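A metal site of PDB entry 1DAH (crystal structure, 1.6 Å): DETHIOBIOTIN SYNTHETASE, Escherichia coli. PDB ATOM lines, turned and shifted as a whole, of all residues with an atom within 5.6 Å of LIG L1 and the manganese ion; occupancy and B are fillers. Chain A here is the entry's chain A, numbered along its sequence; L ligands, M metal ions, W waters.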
ATOM      1  N   ASP A  10       7.076 -25.711  12.719  1.00  0.00           N
ATOM      2  CA  ASP A  10       7.104 -25.710  14.177  1.00  0.00           C
ATOM      3  C   ASP A  10       5.659 -25.975  14.679  1.00  0.00           C
ATOM      4  O   ASP A  10       4.705 -26.036  13.899  1.00  0.00           O
ATOM      5  CB  ASP A  10       7.587 -24.341  14.681  1.00  0.00           C
ATOM      6  CG  ASP A  10       8.111 -24.282  16.122  1.00  0.00           C
ATOM      7  OD1 ASP A  10       8.141 -25.290  16.842  1.00  0.00           O
ATOM      8  OD2 ASP A  10       8.512 -23.208  16.539  1.00  0.00           O
ATOM      9  N   THR A  11       5.512 -26.178  16.004  1.00  0.00           N
ATOM     10  CA  THR A  11       4.223 -26.208  16.674  1.00  0.00           C
ATOM     11  C   THR A  11       3.724 -24.747  16.581  1.00  0.00           C
ATOM     12  O   THR A  11       4.533 -23.813  16.503  1.00  0.00           O
ATOM     13  CB  THR A  11       4.419 -26.690  18.168  1.00  0.00           C
ATOM     14  OG1 THR A  11       3.102 -26.831  18.760  1.00  0.00           O
ATOM     15  CG2 THR A  11       5.290 -25.733  18.995  1.00  0.00           C
ATOM     16  N   GLU A  12       2.421 -24.530  16.531  1.00  0.00           N
ATOM     17  CA  GLU A  12       1.802 -23.212  16.431  1.00  0.00           C
ATOM     18  C   GLU A  12       2.173 -22.425  15.190  1.00  0.00           C
ATOM     19  O   GLU A  12       2.381 -21.221  15.277  1.00  0.00           O
ATOM     20  CB  GLU A  12       2.138 -22.297  17.647  1.00  0.00           C
ATOM     21  CG  GLU A  12       1.835 -22.774  19.071  1.00  0.00           C
ATOM     22  CD  GLU A  12       0.413 -23.256  19.360  1.00  0.00           C
ATOM     23  OE1 GLU A  12      -0.550 -22.653  18.864  1.00  0.00           O
ATOM     24  OE2 GLU A  12       0.293 -24.261  20.063  1.00  0.00           O
ATOM     25  N   VAL A  13       2.252 -22.987  13.983  1.00  0.00           N
ATOM     26  CA  VAL A  13       2.428 -22.163  12.773  1.00  0.00           C
ATOM     27  C   VAL A  13       1.136 -22.055  11.971  1.00  0.00           C
ATOM     28  O   VAL A  13       1.158 -21.540  10.854  1.00  0.00           O
ATOM     29  CB  VAL A  13       3.526 -22.755  11.818  1.00  0.00           C
ATOM     30  CG1 VAL A  13       4.864 -22.519  12.519  1.00  0.00           C
ATOM     31  CG2 VAL A  13       3.338 -24.243  11.511  1.00  0.00           C
ATOM     32  N   GLY A  14       0.002 -22.597  12.429  1.00  0.00           N
ATOM     33  CA  GLY A  14      -1.251 -22.576  11.663  1.00  0.00           C
ATOM     34  C   GLY A  14      -1.566 -23.864  10.936  1.00  0.00           C
ATOM     35  O   GLY A  14      -2.363 -23.886  10.013  1.00  0.00           O
ATOM     36  N   LYS A  15      -1.022 -24.996  11.375  1.00  0.00           N
ATOM     37  CA  LYS A  15      -1.279 -26.271  10.713  1.00  0.00           C
ATOM     38  C   LYS A  15      -2.778 -26.592  10.709  1.00  0.00           C
ATOM     39  O   LYS A  15      -3.272 -27.063   9.685  1.00  0.00           O
ATOM     40  CB  LYS A  15      -0.449 -27.283  11.470  1.00  0.00           C
ATOM     41  CG  LYS A  15      -0.105 -28.634  10.943  1.00  0.00           C
ATOM     42  CD  LYS A  15       0.972 -29.280  11.847  1.00  0.00           C
ATOM     43  CE  LYS A  15       0.605 -29.374  13.344  1.00  0.00           C
ATOM     44  NZ  LYS A  15       1.397 -28.414  14.123  1.00  0.00           N
ATOM     45  N   THR A  16      -3.542 -26.344  11.781  1.00  0.00           N
ATOM     46  CA  THR A  16      -4.970 -26.671  11.695  1.00  0.00           C
ATOM     47  C   THR A  16      -5.706 -25.689  10.798  1.00  0.00           C
ATOM     48  O   THR A  16      -6.612 -26.091  10.081  1.00  0.00           O
ATOM     49  CB  THR A  16      -5.574 -26.697  13.112  1.00  0.00           C
ATOM     50  OG1 THR A  16      -4.815 -27.682  13.830  1.00  0.00           O
ATOM     51  CG2 THR A  16      -7.058 -27.038  13.127  1.00  0.00           C
ATOM     52  N   VAL A  17      -5.246 -24.430  10.708  1.00  0.00           N
ATOM     53  CA  VAL A  17      -5.877 -23.436   9.844  1.00  0.00           C
ATOM     54  C   VAL A  17      -5.686 -23.839   8.392  1.00  0.00           C
ATOM     55  O   VAL A  17      -6.646 -23.841   7.585  1.00  0.00           O
ATOM     56  CB  VAL A  17      -5.266 -21.996  10.137  1.00  0.00           C
ATOM     57  CG1 VAL A  17      -5.737 -20.936   9.117  1.00  0.00           C
ATOM     58  CG2 VAL A  17      -5.752 -21.529  11.520  1.00  0.00           C
ATOM     59  N   ALA A  18      -4.470 -24.246   8.028  1.00  0.00           N
ATOM     60  CA  ALA A  18      -4.231 -24.671   6.664  1.00  0.00           C
ATOM     61  C   ALA A  18      -4.936 -25.995   6.362  1.00  0.00           C
ATOM     62  O   ALA A  18      -5.367 -26.168   5.219  1.00  0.00           O
ATOM     63  CB  ALA A  18      -2.740 -24.826   6.437  1.00  0.00           C
ATOM     64  N   LYS A  37      -6.833 -36.757  12.980  1.00  0.00           N
ATOM     65  CA  LYS A  37      -5.793 -36.262  13.888  1.00  0.00           C
ATOM     66  C   LYS A  37      -5.510 -37.426  14.854  1.00  0.00           C
ATOM     67  O   LYS A  37      -6.159 -37.558  15.892  1.00  0.00           O
ATOM     68  CB  LYS A  37      -6.325 -34.999  14.633  1.00  0.00           C
ATOM     69  CG  LYS A  37      -5.445 -34.406  15.742  1.00  0.00           C
ATOM     70  CD  LYS A  37      -4.628 -33.170  15.368  1.00  0.00           C
ATOM     71  CE  LYS A  37      -3.705 -32.753  16.540  1.00  0.00           C
ATOM     72  NZ  LYS A  37      -2.707 -31.808  16.051  1.00  0.00           N
ATOM     73  N   ASP A  54      -8.320 -28.839  17.799  1.00  0.00           N
ATOM     74  CA  ASP A  54      -7.873 -29.140  16.443  1.00  0.00           C
ATOM     75  C   ASP A  54      -8.712 -30.241  15.830  1.00  0.00           C
ATOM     76  O   ASP A  54      -9.250 -30.095  14.735  1.00  0.00           O
ATOM     77  CB  ASP A  54      -6.426 -29.626  16.430  1.00  0.00           C
ATOM     78  CG  ASP A  54      -5.326 -28.631  16.807  1.00  0.00           C
ATOM     79  OD1 ASP A  54      -5.583 -27.428  17.009  1.00  0.00           O
ATOM     80  OD2 ASP A  54      -4.201 -29.084  16.853  1.00  0.00           O
ATOM     81  N   GLU A 115      -3.417 -34.950  10.110  1.00  0.00           N
ATOM     82  CA  GLU A 115      -2.656 -33.862  10.714  1.00  0.00           C
ATOM     83  C   GLU A 115      -1.790 -34.500  11.784  1.00  0.00           C
ATOM     84  O   GLU A 115      -2.264 -35.318  12.576  1.00  0.00           O
ATOM     85  CB  GLU A 115      -3.609 -32.820  11.327  1.00  0.00           C
ATOM     86  CG  GLU A 115      -2.917 -31.563  11.781  1.00  0.00           C
ATOM     87  CD  GLU A 115      -3.748 -30.492  12.475  1.00  0.00           C
ATOM     88  OE1 GLU A 115      -4.730 -30.029  11.907  1.00  0.00           O
ATOM     89  OE2 GLU A 115      -3.378 -30.079  13.584  1.00  0.00           O
ATOM     90  N   GLY A 116      -0.493 -34.238  11.810  1.00  0.00           N
ATOM     91  CA  GLY A 116       0.332 -34.766  12.868  1.00  0.00           C
ATOM     92  C   GLY A 116       0.240 -33.915  14.128  1.00  0.00           C
ATOM     93  O   GLY A 116      -0.614 -33.017  14.293  1.00  0.00           O
ATOM     94  N   ALA A 117       1.133 -34.205  15.060  1.00  0.00           N
ATOM     95  CA  ALA A 117       1.205 -33.370  16.253  1.00  0.00           C
ATOM     96  C   ALA A 117       2.571 -32.685  16.243  1.00  0.00           C
ATOM     97  O   ALA A 117       3.555 -33.380  15.956  1.00  0.00           O
ATOM     98  CB  ALA A 117       1.033 -34.213  17.512  1.00  0.00           C
ATOM     99  N   GLY A 118       2.643 -31.380  16.546  1.00  0.00           N
ATOM    100  CA  GLY A 118       3.912 -30.637  16.582  1.00  0.00           C
ATOM    101  C   GLY A 118       4.575 -30.569  15.196  1.00  0.00           C
ATOM    102  O   GLY A 118       3.888 -30.339  14.182  1.00  0.00           O
ATOM    103  N   ASN A 175       1.488 -19.644   5.493  1.00  0.00           N
ATOM    104  CA  ASN A 175       0.496 -19.138   6.408  1.00  0.00           C
ATOM    105  C   ASN A 175       0.962 -17.830   7.068  1.00  0.00           C
ATOM    106  O   ASN A 175       2.013 -17.787   7.713  1.00  0.00           O
ATOM    107  CB  ASN A 175       0.203 -20.184   7.463  1.00  0.00           C
ATOM    108  CG  ASN A 175      -0.974 -19.788   8.332  1.00  0.00           C
ATOM    109  OD1 ASN A 175      -1.902 -19.102   7.921  1.00  0.00           O
ATOM    110  ND2 ASN A 175      -1.055 -20.166   9.590  1.00  0.00           N
ATOM    111  N   ASP A 176       0.244 -16.737   6.852  1.00  0.00           N
ATOM    112  CA  ASP A 176       0.650 -15.472   7.445  1.00  0.00           C
ATOM    113  C   ASP A 176       0.191 -15.320   8.876  1.00  0.00           C
ATOM    114  O   ASP A 176      -0.923 -14.942   9.195  1.00  0.00           O
ATOM    115  CB  ASP A 176       0.105 -14.333   6.628  1.00  0.00           C
ATOM    116  CG  ASP A 176       0.543 -14.372   5.178  1.00  0.00           C
ATOM    117  OD1 ASP A 176       1.550 -15.004   4.828  1.00  0.00           O
ATOM    118  OD2 ASP A 176      -0.126 -13.755   4.372  1.00  0.00           O
ATOM    119  N   VAL A 177       1.092 -15.700   9.748  1.00  0.00           N
ATOM    120  CA  VAL A 177       0.839 -15.685  11.178  1.00  0.00           C
ATOM    121  C   VAL A 177       0.947 -14.260  11.739  1.00  0.00           C
ATOM    122  O   VAL A 177       0.456 -14.047  12.844  1.00  0.00           O
ATOM    123  CB  VAL A 177       1.810 -16.657  11.906  1.00  0.00           C
ATOM    124  CG1 VAL A 177       1.459 -18.043  11.386  1.00  0.00           C
ATOM    125  CG2 VAL A 177       3.288 -16.389  11.667  1.00  0.00           C
ATOM    126  N   ILE A 203      -2.369 -18.277   2.937  1.00  0.00           N
ATOM    127  CA  ILE A 203      -3.506 -17.843   3.735  1.00  0.00           C
ATOM    128  C   ILE A 203      -3.102 -16.530   4.412  1.00  0.00           C
ATOM    129  O   ILE A 203      -2.053 -16.445   5.091  1.00  0.00           O
ATOM    130  CB  ILE A 203      -3.811 -18.966   4.734  1.00  0.00           C
ATOM    131  CG1 ILE A 203      -4.188 -20.241   3.956  1.00  0.00           C
ATOM    132  CG2 ILE A 203      -4.947 -18.550   5.666  1.00  0.00           C
ATOM    133  CD1 ILE A 203      -4.054 -21.503   4.817  1.00  0.00           C
ATOM    134  N   PRO A 204      -3.881 -15.453   4.202  1.00  0.00           N
ATOM    135  CA  PRO A 204      -3.599 -14.135   4.791  1.00  0.00           C
ATOM    136  C   PRO A 204      -3.823 -14.134   6.298  1.00  0.00           C
ATOM    137  O   PRO A 204      -4.461 -15.063   6.843  1.00  0.00           O
ATOM    138  CB  PRO A 204      -4.531 -13.204   4.037  1.00  0.00           C
ATOM    139  CG  PRO A 204      -5.698 -14.063   3.685  1.00  0.00           C
ATOM    140  CD  PRO A 204      -5.096 -15.436   3.418  1.00  0.00           C
ATOM    141  N   TRP A 205      -3.316 -13.094   6.976  1.00  0.00           N
ATOM    142  CA  TRP A 205      -3.423 -12.953   8.417  1.00  0.00           C
ATOM    143  C   TRP A 205      -4.893 -12.669   8.675  1.00  0.00           C
ATOM    144  O   TRP A 205      -5.487 -11.747   8.083  1.00  0.00           O
ATOM    145  CB  TRP A 205      -2.533 -11.765   8.920  1.00  0.00           C
ATOM    146  CG  TRP A 205      -2.734 -11.398  10.394  1.00  0.00           C
ATOM    147  CD1 TRP A 205      -2.332 -12.256  11.388  1.00  0.00           C
ATOM    148  CD2 TRP A 205      -3.360 -10.279  10.881  1.00  0.00           C
ATOM    149  NE1 TRP A 205      -2.700 -11.677  12.500  1.00  0.00           N
ATOM    150  CE2 TRP A 205      -3.310 -10.513  12.261  1.00  0.00           C
ATOM    151  CE3 TRP A 205      -3.972  -9.107  10.407  1.00  0.00           C
ATOM    152  CZ2 TRP A 205      -3.862  -9.573  13.153  1.00  0.00           C
ATOM    153  CZ3 TRP A 205      -4.515  -8.180  11.289  1.00  0.00           C
ATOM    154  CH2 TRP A 205      -4.464  -8.418  12.655  1.00  0.00           C
ATOM    155  N   LEU A 206      -5.554 -13.441   9.510  1.00  0.00           N
ATOM    156  CA  LEU A 206      -6.971 -13.247   9.784  1.00  0.00           C
ATOM    157  C   LEU A 206      -7.021 -13.161  11.306  1.00  0.00           C
ATOM    158  O   LEU A 206      -6.783 -14.116  12.035  1.00  0.00           O
ATOM    159  CB  LEU A 206      -7.772 -14.446   9.238  1.00  0.00           C
ATOM    160  CG  LEU A 206      -7.729 -14.592   7.714  1.00  0.00           C
ATOM    161  CD1 LEU A 206      -7.949 -16.046   7.318  1.00  0.00           C
ATOM    162  CD2 LEU A 206      -8.712 -13.605   7.105  1.00  0.00           C
ATOM    163  N   ALA A 207      -7.242 -11.959  11.779  1.00  0.00           N
ATOM    164  CA  ALA A 207      -7.321 -11.721  13.208  1.00  0.00           C
ATOM    165  C   ALA A 207      -8.276 -12.638  13.991  1.00  0.00           C
ATOM    166  O   ALA A 207      -7.827 -13.445  14.810  1.00  0.00           O
ATOM    167  CB  ALA A 207      -7.737 -10.258  13.380  1.00  0.00           C
ATOM    168  N   ASN A 209     -10.617 -15.707  14.773  1.00  0.00           N
ATOM    169  CA  ASN A 209     -11.009 -17.073  14.506  1.00  0.00           C
ATOM    170  C   ASN A 209     -10.764 -17.771  13.136  1.00  0.00           C
ATOM    171  O   ASN A 209     -11.664 -18.457  12.611  1.00  0.00           O
ATOM    172  CB  ASN A 209     -12.507 -17.174  14.861  1.00  0.00           C
ATOM    173  CG  ASN A 209     -12.780 -18.230  15.927  1.00  0.00           C
ATOM    174  OD1 ASN A 209     -12.346 -19.376  15.832  1.00  0.00           O
ATOM    175  ND2 ASN A 209     -13.539 -17.887  16.971  1.00  0.00           N
ATOM    176  N   PRO A 210      -9.538 -17.778  12.571  1.00  0.00           N
ATOM    177  CA  PRO A 210      -9.274 -18.156  11.183  1.00  0.00           C
ATOM    178  C   PRO A 210      -9.646 -19.584  10.794  1.00  0.00           C
ATOM    179  O   PRO A 210      -9.848 -19.878   9.613  1.00  0.00           O
ATOM    180  CB  PRO A 210      -7.789 -17.854  11.017  1.00  0.00           C
ATOM    181  CG  PRO A 210      -7.215 -18.086  12.401  1.00  0.00           C
ATOM    182  CD  PRO A 210      -8.291 -17.433  13.257  1.00  0.00           C
ATOM    183  N   GLU A 211      -9.779 -20.500  11.774  1.00  0.00           N
ATOM    184  CA  GLU A 211     -10.175 -21.895  11.506  1.00  0.00           C
ATOM    185  C   GLU A 211     -11.669 -22.039  11.145  1.00  0.00           C
ATOM    186  O   GLU A 211     -12.085 -23.032  10.499  1.00  0.00           O
ATOM    187  CB  GLU A 211      -9.803 -22.804  12.726  1.00  0.00           C
ATOM    188  CG  GLU A 211     -10.056 -22.400  14.181  1.00  0.00           C
ATOM    189  CD  GLU A 211      -9.290 -21.172  14.697  1.00  0.00           C
ATOM    190  OE1 GLU A 211      -8.050 -21.161  14.875  1.00  0.00           O
ATOM    191  OE2 GLU A 211      -9.974 -20.178  14.932  1.00  0.00           O
HETATM  192  P1  LIG L   1      -0.384 -27.454  17.201  1.00  0.00           P
HETATM  193  O1  LIG L   1       1.103 -27.646  17.185  1.00  0.00           O
HETATM  194  O2  LIG L   1      -1.040 -28.485  16.150  1.00  0.00           O
HETATM  195  O3  LIG L   1      -0.955 -27.588  18.563  1.00  0.00           O
HETATM  196  P2  LIG L   1      -0.939 -25.510  14.695  1.00  0.00           P
HETATM  197  O4  LIG L   1      -1.848 -26.554  14.152  1.00  0.00           O
HETATM  198  O5  LIG L   1       0.443 -25.567  14.121  1.00  0.00           O
HETATM  199  C1  LIG L   1      -0.846 -25.823  16.508  1.00  0.00           C
HETATM  200  P3  LIG L   1      -3.134 -23.557  14.474  1.00  0.00           P
HETATM  201  O6  LIG L   1      -3.893 -24.208  15.566  1.00  0.00           O
HETATM  202  O7  LIG L   1      -3.795 -23.737  13.151  1.00  0.00           O
HETATM  203  O8  LIG L   1      -1.618 -24.111  14.422  1.00  0.00           O
HETATM  204  O9  LIG L   1      -2.906 -22.001  14.797  1.00  0.00           O
HETATM  205  C2  LIG L   1      -2.022 -21.612  15.864  1.00  0.00           C
HETATM  206  C3  LIG L   1      -2.460 -20.249  16.389  1.00  0.00           C
HETATM  207  O10 LIG L   1      -2.114 -19.253  15.406  1.00  0.00           O
HETATM  208  C4  LIG L   1      -3.963 -20.167  16.609  1.00  0.00           C
HETATM  209  O11 LIG L   1      -4.282 -19.308  17.708  1.00  0.00           O
HETATM  210  C5  LIG L   1      -4.472 -19.636  15.274  1.00  0.00           C
HETATM  211  O12 LIG L   1      -5.805 -19.105  15.284  1.00  0.00           O
HETATM  212  C6  LIG L   1      -3.338 -18.680  14.900  1.00  0.00           C
HETATM  213  N1  LIG L   1      -3.177 -18.533  13.422  1.00  0.00           N
HETATM  214  C7  LIG L   1      -2.836 -19.498  12.572  1.00  0.00           C
HETATM  215  N2  LIG L   1      -2.979 -19.025  11.337  1.00  0.00           N
HETATM  216  C8  LIG L   1      -3.403 -17.775  11.395  1.00  0.00           C
HETATM  217  C9  LIG L   1      -3.726 -16.798  10.439  1.00  0.00           C
HETATM  218  N3  LIG L   1      -3.795 -17.085   9.156  1.00  0.00           N
HETATM  219  N4  LIG L   1      -4.105 -15.581  10.891  1.00  0.00           N
HETATM  220  C10 LIG L   1      -4.184 -15.305  12.196  1.00  0.00           C
HETATM  221  N5  LIG L   1      -3.915 -16.230  13.095  1.00  0.00           N
HETATM  222  C11 LIG L   1      -3.522 -17.455  12.739  1.00  0.00           C
HETATM  223  C1  LG2 L   2       8.786 -31.210  20.611  1.00  0.00           C
HETATM  224  O1  LG2 L   2       9.317 -30.578  21.531  1.00  0.00           O
HETATM  225  O2  LG2 L   2       9.269 -31.221  19.478  1.00  0.00           O
HETATM  226  C2  LG2 L   2       7.446 -31.923  20.847  1.00  0.00           C
HETATM  227  C3  LG2 L   2       6.305 -30.934  20.546  1.00  0.00           C
HETATM  228  C4  LG2 L   2       4.906 -31.524  20.664  1.00  0.00           C
HETATM  229  C5  LG2 L   2       3.887 -30.427  20.377  1.00  0.00           C
HETATM  230  C6  LG2 L   2       2.480 -30.973  20.485  1.00  0.00           C
HETATM  231  C7  LG2 L   2       1.279 -30.021  20.311  1.00  0.00           C
HETATM  232  C8  LG2 L   2       1.325 -28.867  21.363  1.00  0.00           C
HETATM  233  C9  LG2 L   2       1.052 -29.390  22.763  1.00  0.00           C
HETATM  234  N1  LG2 L   2       0.097 -30.841  20.522  1.00  0.00           N
HETATM  235  N2  LG2 L   2       0.363 -27.818  21.075  1.00  0.00           N
HETATM  236 MN    MN M   1      -2.939 -28.197  15.148  1.00  0.00          MN
HETATM  237  O   HOH W   1      -3.352 -29.490  19.467  1.00  0.00           O
HETATM  238  O   HOH W   2      -0.257 -30.680  17.587  1.00  0.00           O
HETATM  239  O   HOH W   3      -6.580 -23.895  14.544  1.00  0.00           O
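N of Thr 16 lies within hydrogen-bond range of O7 of LIG L1 (3.0 Å). The side-chain hydroxyl (OG1) of Thr 11 sits at hydrogen-bond distance from an oxygen (O1) of LIG L1, at 2.7 Å. N2 of LIG L1 is in hydrogen-bond range of ND2 of Asn 175 (2.8 Å). The backbone NH of Leu 206 sits at hydrogen-bond distance from a nitrogen (N4) of LIG L1, at 2.9 Å. An oxygen (O7) of LIG L1 lies within hydrogen-bond range of the backbone NH of Val 17. The backbone NH of Gly 14 lies within hydrogen-bond range of an oxygen (O8) of LIG L1 (3.0 Å). N of Lys 15 sits at hydrogen-bond distance from O5 of LIG L1, at 3.2 Å. NZ of Lys 15 is in salt-bridge range of O5 of LIG L1 (3.0 Å). The side-chain carboxylate of Glu 211 sits at hydrogen-bond distance from an oxygen (O12) of LIG L1. A nitrogen (N3) of LIG L1 lies within hydrogen-bond range of the backbone carbonyl oxygen (O) of Pro 204. The backbone NH (N) of Val 13 lies within hydrogen-bond range of an oxygen (O5) of LIG L1, at 3.2 Å. The backbone NH (N) of Glu 12 sits at hydrogen-bond distance from an oxygen (O5) of LIG L1 (3.3 Å). NZ of Lys 37 lies close to O2 of LIG L1, 3.7 Å away. A nitrogen (N2) of LG2 L2 lies within salt-bridge range of the side-chain carboxylate of Glu 12.
Water W2 lies within hydrogen-bond range of a nitrogen (N1) of LG2 L2 (3.0 Å), the side-chain amino group (NZ) of Lys 37 (3.1 Å), the backbone NH (N) of Gly 118 (3.2 Å) and an oxygen (O3) of LIG L1 (3.3 Å). Water W3 bridges O6 of LIG L1 (2.9 Å) and OE1 of Glu 211 (3.1 Å).
O of Asp 176 touches N3 of LIG L1, 3.6 Å away. Ile 203 touches LIG L1 (CG2 to N3, 3.96 Å). Trp 205 touches LIG L1 (CD1 to C10, 3.7 Å). CG of Pro 210 touches O12 of LIG L1 (3.4 Å). Hydrophobic or aromatic side chains within 4 Å of LIG L1: Val 17, Ile 203, Trp 205 and Pro 210. Within 4 Å of LIG L1: Thr 11, Glu 12, Val 13, Gly 14, Lys 15, Thr 16, Val 17, Lys 37, Asp 54, Glu 115, Asn 175, Asp 176, Ile 203, Pro 204, Trp 205, Leu 206, Pro 210 and Glu 211. Along chain A the residues within 4 Å of LIG L1 span positions 11 to 211.
The manganese ion is bound by O2 of LIG L1, O4 of LIG L1, OD2 of Asp 54, OG1 of Thr 16 and OE2 of Glu 115. The manganese ion has five donor atoms within binding distance.
Merely in contact with the manganese ion: Lys 37 (3.7 Å).
A nitrogen (N2) of LG2 L2 is in hydrogen-bond range of an oxygen (O3) of LIG L1 (2.8 Å).
The side-chain carboxylate (OD2) of Asp 54 sits close to the side-chain amino group (NZ) of Lys 37 (3.2 Å). The side-chain amino group (NZ) of Lys 37 lies close to the side-chain carboxylate (OE2) of Glu 115 (3.1 Å). The backbone carbonyl oxygen (O) of Val 13 sits at hydrogen-bond distance from the side-chain amide nitrogen (ND2) of Asn 175 (2.9 Å). The backbone carbonyl oxygen (O) of Gly 118 lies within hydrogen-bond range of the side-chain amino group (NZ) of Lys 15, at 3.1 Å. OD1 of Asn 209 lies close to OE2 of Glu 211, at 2.7 Å. The backbone NH (N) of Asp 176 sits at hydrogen-bond distance from the backbone carbonyl oxygen (O) of Ile 203 (2.9 Å). The side-chain amino group of Lys 37 lies within hydrogen-bond range of the backbone carbonyl oxygen of Gly 116 (3.0 Å).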
